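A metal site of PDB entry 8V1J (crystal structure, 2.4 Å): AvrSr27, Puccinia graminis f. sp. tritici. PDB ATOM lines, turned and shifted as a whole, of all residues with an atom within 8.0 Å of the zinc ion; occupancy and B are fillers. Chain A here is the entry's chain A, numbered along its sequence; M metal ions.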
ATOM      1  N   GLY A  23      13.907 -16.912 -15.370  1.00  0.00           N
ATOM      2  CA  GLY A  23      12.575 -16.724 -14.841  1.00  0.00           C
ATOM      3  C   GLY A  23      12.582 -16.512 -13.348  1.00  0.00           C
ATOM      4  O   GLY A  23      13.651 -16.295 -12.754  1.00  0.00           O
ATOM      5  N   LYS A  24      11.410 -16.565 -12.714  1.00  0.00           N
ATOM      6  CA  LYS A  24      11.309 -16.344 -11.281  1.00  0.00           C
ATOM      7  C   LYS A  24      11.658 -17.614 -10.524  1.00  0.00           C
ATOM      8  O   LYS A  24      11.068 -18.676 -10.774  1.00  0.00           O
ATOM      9  CB  LYS A  24       9.905 -15.871 -10.915  1.00  0.00           C
ATOM     10  CG  LYS A  24       9.641 -15.825  -9.414  1.00  0.00           C
ATOM     11  CD  LYS A  24       8.317 -15.141  -9.103  1.00  0.00           C
ATOM     12  CE  LYS A  24       7.892 -15.385  -7.659  1.00  0.00           C
ATOM     13  NZ  LYS A  24       6.867 -14.411  -7.195  1.00  0.00           N
ATOM     14  N   CYS A  25      12.614 -17.520  -9.605  1.00  0.00           N
ATOM     15  CA  CYS A  25      12.898 -18.621  -8.696  1.00  0.00           C
ATOM     16  C   CYS A  25      11.806 -18.717  -7.644  1.00  0.00           C
ATOM     17  O   CYS A  25      11.465 -17.721  -7.001  1.00  0.00           O
ATOM     18  CB  CYS A  25      14.267 -18.424  -8.030  1.00  0.00           C
ATOM     19  SG  CYS A  25      14.619 -19.569  -6.660  1.00  0.00           S
ATOM     20  N   ASP A  26      11.249 -19.917  -7.473  1.00  0.00           N
ATOM     21  CA  ASP A  26      10.154 -20.081  -6.522  1.00  0.00           C
ATOM     22  C   ASP A  26      10.615 -19.890  -5.093  1.00  0.00           C
ATOM     23  O   ASP A  26       9.802 -19.510  -4.230  1.00  0.00           O
ATOM     24  CB  ASP A  26       9.519 -21.460  -6.699  1.00  0.00           C
ATOM     25  CG  ASP A  26       8.550 -21.520  -7.858  1.00  0.00           C
ATOM     26  OD1 ASP A  26       7.858 -20.512  -8.110  1.00  0.00           O
ATOM     27  OD2 ASP A  26       8.474 -22.582  -8.516  1.00  0.00           O
ATOM     28  N   SER A  27      11.893 -20.134  -4.805  1.00  0.00           N
ATOM     29  CA  SER A  27      12.392 -20.038  -3.434  1.00  0.00           C
ATOM     30  C   SER A  27      12.602 -18.585  -3.007  1.00  0.00           C
ATOM     31  O   SER A  27      11.921 -18.078  -2.114  1.00  0.00           O
ATOM     32  CB  SER A  27      13.678 -20.851  -3.298  1.00  0.00           C
ATOM     33  OG  SER A  27      13.447 -22.217  -3.574  1.00  0.00           O
ATOM     34  N   CYS A  28      13.556 -17.900  -3.648  1.00  0.00           N
ATOM     35  CA  CYS A  28      13.833 -16.512  -3.278  1.00  0.00           C
ATOM     36  C   CYS A  28      12.875 -15.523  -3.922  1.00  0.00           C
ATOM     37  O   CYS A  28      12.782 -14.387  -3.457  1.00  0.00           O
ATOM     38  CB  CYS A  28      15.278 -16.145  -3.659  1.00  0.00           C
ATOM     39  SG  CYS A  28      15.648 -16.128  -5.430  1.00  0.00           S
ATOM     40  N   GLN A  29      12.142 -15.940  -4.956  1.00  0.00           N
ATOM     41  CA  GLN A  29      11.156 -15.122  -5.649  1.00  0.00           C
ATOM     42  C   GLN A  29      11.780 -14.004  -6.479  1.00  0.00           C
ATOM     43  O   GLN A  29      11.069 -13.084  -6.912  1.00  0.00           O
ATOM     44  CB  GLN A  29      10.126 -14.531  -4.673  1.00  0.00           C
ATOM     45  CG  GLN A  29       9.456 -15.575  -3.807  1.00  0.00           C
ATOM     46  CD  GLN A  29       8.303 -15.022  -2.998  1.00  0.00           C
ATOM     47  OE1 GLN A  29       7.641 -14.079  -3.422  1.00  0.00           O
ATOM     48  NE2 GLN A  29       8.058 -15.610  -1.835  1.00  0.00           N
ATOM     49  N   LEU A  30      13.084 -14.061  -6.722  1.00  0.00           N
ATOM     50  CA  LEU A  30      13.740 -13.117  -7.606  1.00  0.00           C
ATOM     51  C   LEU A  30      13.822 -13.687  -9.015  1.00  0.00           C
ATOM     52  O   LEU A  30      13.689 -14.894  -9.227  1.00  0.00           O
ATOM     53  CB  LEU A  30      15.135 -12.773  -7.076  1.00  0.00           C
ATOM     54  CG  LEU A  30      15.146 -12.025  -5.743  1.00  0.00           C
ATOM     55  CD1 LEU A  30      16.468 -12.236  -5.027  1.00  0.00           C
ATOM     56  CD2 LEU A  30      14.887 -10.552  -5.967  1.00  0.00           C
ATOM     57  N   HIS A  31      14.033 -12.796  -9.986  1.00  0.00           N
ATOM     58  CA  HIS A  31      14.073 -13.178 -11.398  1.00  0.00           C
ATOM     59  C   HIS A  31      15.478 -13.693 -11.737  1.00  0.00           C
ATOM     60  O   HIS A  31      16.232 -13.108 -12.508  1.00  0.00           O
ATOM     61  CB  HIS A  31      13.692 -11.984 -12.265  1.00  0.00           C
ATOM     62  CG  HIS A  31      13.440 -12.326 -13.699  1.00  0.00           C
ATOM     63  ND1 HIS A  31      12.265 -12.887 -14.129  1.00  0.00           N
ATOM     64  CD2 HIS A  31      14.211 -12.184 -14.795  1.00  0.00           C
ATOM     65  CE1 HIS A  31      12.321 -13.086 -15.436  1.00  0.00           C
ATOM     66  NE2 HIS A  31      13.493 -12.663 -15.867  1.00  0.00           N
ATOM     67  N   THR A  32      15.815 -14.832 -11.117  1.00  0.00           N
ATOM     68  CA  THR A  32      17.161 -15.367 -11.169  1.00  0.00           C
ATOM     69  C   THR A  32      17.208 -16.865 -11.447  1.00  0.00           C
ATOM     70  O   THR A  32      18.283 -17.478 -11.326  1.00  0.00           O
ATOM     71  CB  THR A  32      17.902 -15.084  -9.855  1.00  0.00           C
ATOM     72  OG1 THR A  32      17.075 -15.485  -8.740  1.00  0.00           O
ATOM     73  CG2 THR A  32      18.232 -13.609  -9.727  1.00  0.00           C
ATOM     74  N   LYS A  33      16.085 -17.488 -11.814  1.00  0.00           N
ATOM     75  CA  LYS A  33      16.038 -18.922 -12.080  1.00  0.00           C
ATOM     76  C   LYS A  33      16.324 -19.181 -13.558  1.00  0.00           C
ATOM     77  O   LYS A  33      15.575 -18.725 -14.425  1.00  0.00           O
ATOM     78  CB  LYS A  33      14.675 -19.490 -11.696  1.00  0.00           C
ATOM     79  CG  LYS A  33      14.455 -20.928 -12.165  1.00  0.00           C
ATOM     80  CD  LYS A  33      13.087 -21.425 -11.750  1.00  0.00           C
ATOM     81  CE  LYS A  33      12.905 -22.877 -12.148  1.00  0.00           C
ATOM     82  NZ  LYS A  33      11.627 -23.430 -11.633  1.00  0.00           N
ATOM     83  N   GLU A  52      18.893 -23.795 -12.154  1.00  0.00           N
ATOM     84  CA  GLU A  52      19.744 -23.171 -11.152  1.00  0.00           C
ATOM     85  C   GLU A  52      19.241 -21.763 -10.884  1.00  0.00           C
ATOM     86  O   GLU A  52      18.731 -21.094 -11.778  1.00  0.00           O
ATOM     87  CB  GLU A  52      21.209 -23.128 -11.585  1.00  0.00           C
ATOM     88  CG  GLU A  52      21.489 -22.232 -12.801  1.00  0.00           C
ATOM     89  CD  GLU A  52      22.970 -22.044 -13.066  1.00  0.00           C
ATOM     90  OE1 GLU A  52      23.784 -22.771 -12.461  1.00  0.00           O
ATOM     91  OE2 GLU A  52      23.317 -21.163 -13.876  1.00  0.00           O
ATOM     92  N   CYS A  53      19.383 -21.331  -9.627  1.00  0.00           N
ATOM     93  CA  CYS A  53      19.159 -19.952  -9.251  1.00  0.00           C
ATOM     94  C   CYS A  53      20.505 -19.283  -9.017  1.00  0.00           C
ATOM     95  O   CYS A  53      21.424 -19.890  -8.447  1.00  0.00           O
ATOM     96  CB  CYS A  53      18.298 -19.842  -7.987  1.00  0.00           C
ATOM     97  SG  CYS A  53      18.097 -18.150  -7.368  1.00  0.00           S
ATOM     98  N   SER A  54      20.637 -18.030  -9.455  1.00  0.00           N
ATOM     99  CA  SER A  54      21.871 -17.287  -9.300  1.00  0.00           C
ATOM    100  C   SER A  54      21.941 -16.506  -7.993  1.00  0.00           C
ATOM    101  O   SER A  54      22.968 -15.886  -7.714  1.00  0.00           O
ATOM    102  CB  SER A  54      22.066 -16.334 -10.482  1.00  0.00           C
ATOM    103  OG  SER A  54      20.948 -15.475 -10.633  1.00  0.00           O
ATOM    104  N   THR A  55      20.883 -16.536  -7.192  1.00  0.00           N
ATOM    105  CA  THR A  55      20.867 -15.794  -5.938  1.00  0.00           C
ATOM    106  C   THR A  55      21.764 -16.472  -4.918  1.00  0.00           C
ATOM    107  O   THR A  55      21.603 -17.660  -4.614  1.00  0.00           O
ATOM    108  CB  THR A  55      19.439 -15.676  -5.407  1.00  0.00           C
ATOM    109  OG1 THR A  55      18.592 -15.157  -6.437  1.00  0.00           O
ATOM    110  CG2 THR A  55      19.393 -14.735  -4.204  1.00  0.00           C
ATOM    111  N   LYS A  56      22.714 -15.716  -4.376  1.00  0.00           N
ATOM    112  CA  LYS A  56      23.633 -16.243  -3.372  1.00  0.00           C
ATOM    113  C   LYS A  56      22.878 -16.587  -2.097  1.00  0.00           C
ATOM    114  O   LYS A  56      22.159 -15.761  -1.535  1.00  0.00           O
ATOM    115  CB  LYS A  56      24.715 -15.201  -3.085  1.00  0.00           C
ATOM    116  CG  LYS A  56      25.854 -15.663  -2.192  1.00  0.00           C
ATOM    117  CD  LYS A  56      26.712 -14.461  -1.801  1.00  0.00           C
ATOM    118  CE  LYS A  56      28.192 -14.808  -1.673  1.00  0.00           C
ATOM    119  NZ  LYS A  56      29.029 -13.576  -1.614  1.00  0.00           N
ATOM    120  N   GLY A  57      23.036 -17.831  -1.643  1.00  0.00           N
ATOM    121  CA  GLY A  57      22.381 -18.295  -0.439  1.00  0.00           C
ATOM    122  C   GLY A  57      21.009 -18.896  -0.630  1.00  0.00           C
ATOM    123  O   GLY A  57      20.435 -19.405   0.334  1.00  0.00           O
ATOM    124  N   CYS A  58      20.467 -18.851  -1.849  1.00  0.00           N
ATOM    125  CA  CYS A  58      19.156 -19.432  -2.093  1.00  0.00           C
ATOM    126  C   CYS A  58      19.266 -20.956  -2.109  1.00  0.00           C
ATOM    127  O   CYS A  58      20.210 -21.506  -2.676  1.00  0.00           O
ATOM    128  CB  CYS A  58      18.590 -18.924  -3.419  1.00  0.00           C
ATOM    129  SG  CYS A  58      16.935 -19.521  -3.831  1.00  0.00           S
ATOM    130  N   PRO A  59      18.315 -21.675  -1.490  1.00  0.00           N
ATOM    131  CA  PRO A  59      18.374 -23.144  -1.548  1.00  0.00           C
ATOM    132  C   PRO A  59      18.404 -23.689  -2.972  1.00  0.00           C
ATOM    133  O   PRO A  59      18.927 -24.792  -3.195  1.00  0.00           O
ATOM    134  CB  PRO A  59      17.101 -23.575  -0.816  1.00  0.00           C
ATOM    135  CG  PRO A  59      16.783 -22.444   0.086  1.00  0.00           C
ATOM    136  CD  PRO A  59      17.206 -21.199  -0.647  1.00  0.00           C
ATOM    137  N   ALA A  60      17.842 -22.958  -3.930  1.00  0.00           N
ATOM    138  CA  ALA A  60      17.844 -23.370  -5.330  1.00  0.00           C
ATOM    139  C   ALA A  60      19.163 -23.065  -6.036  1.00  0.00           C
ATOM    140  O   ALA A  60      19.302 -23.391  -7.216  1.00  0.00           O
ATOM    141  CB  ALA A  60      16.687 -22.702  -6.076  1.00  0.00           C
ATOM    142  N   ASN A  61      20.115 -22.448  -5.335  1.00  0.00           N
ATOM    143  CA  ASN A  61      21.465 -22.274  -5.845  1.00  0.00           C
ATOM    144  C   ASN A  61      22.318 -23.428  -5.344  1.00  0.00           C
ATOM    145  O   ASN A  61      22.449 -23.626  -4.128  1.00  0.00           O
ATOM    146  CB  ASN A  61      22.032 -20.921  -5.402  1.00  0.00           C
ATOM    147  CG  ASN A  61      23.419 -20.651  -5.972  1.00  0.00           C
ATOM    148  OD1 ASN A  61      24.138 -21.560  -6.388  1.00  0.00           O
ATOM    149  ND2 ASN A  61      23.796 -19.381  -5.991  1.00  0.00           N
HETATM  150 ZN    ZN M   1      16.481 -18.351  -5.755  1.00  0.00          ZN
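The side-chain hydroxyl (OG1) of Thr 55 sits close to the side-chain sulfur (SG) of Cys 28 (3.3 Å). The backbone NH (N) of Cys 53 sits at hydrogen-bond distance from the backbone carbonyl oxygen (O) of Ala 60, at 3.2 Å. SG of Cys 28 sits close to N of Leu 30 (3.5 Å). SG of Cys 53 lies close to OG1 of Thr 32 (3.2 Å). N of Cys 25 sits at hydrogen-bond distance from O of Leu 30 (2.9 Å). N of Ala 60 sits close to SG of Cys 58 (3.6 Å). ND2 of Asn 61 is in hydrogen-bond range of O of Thr 55, 3.1 Å away. The side-chain sulfur of Cys 28 lies close to the side-chain hydroxyl of Thr 32, at 3.7 Å.
The zinc ion is bound by SG of Cys 53 (2.3 Å), SG of Cys 58 (2.3 Å), SG of Cys 28 (2.4 Å) and SG of Cys 25 (2.4 Å). The zinc ion has four donor atoms within binding distance.
Residues that only touch the zinc ion: Thr 55 (3.9 Å). Of the 21 residues printed, 5 come within 4 Å of the zinc ion. Along chain A the residues within 4 Å of the zinc ion span positions 25 to 58.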
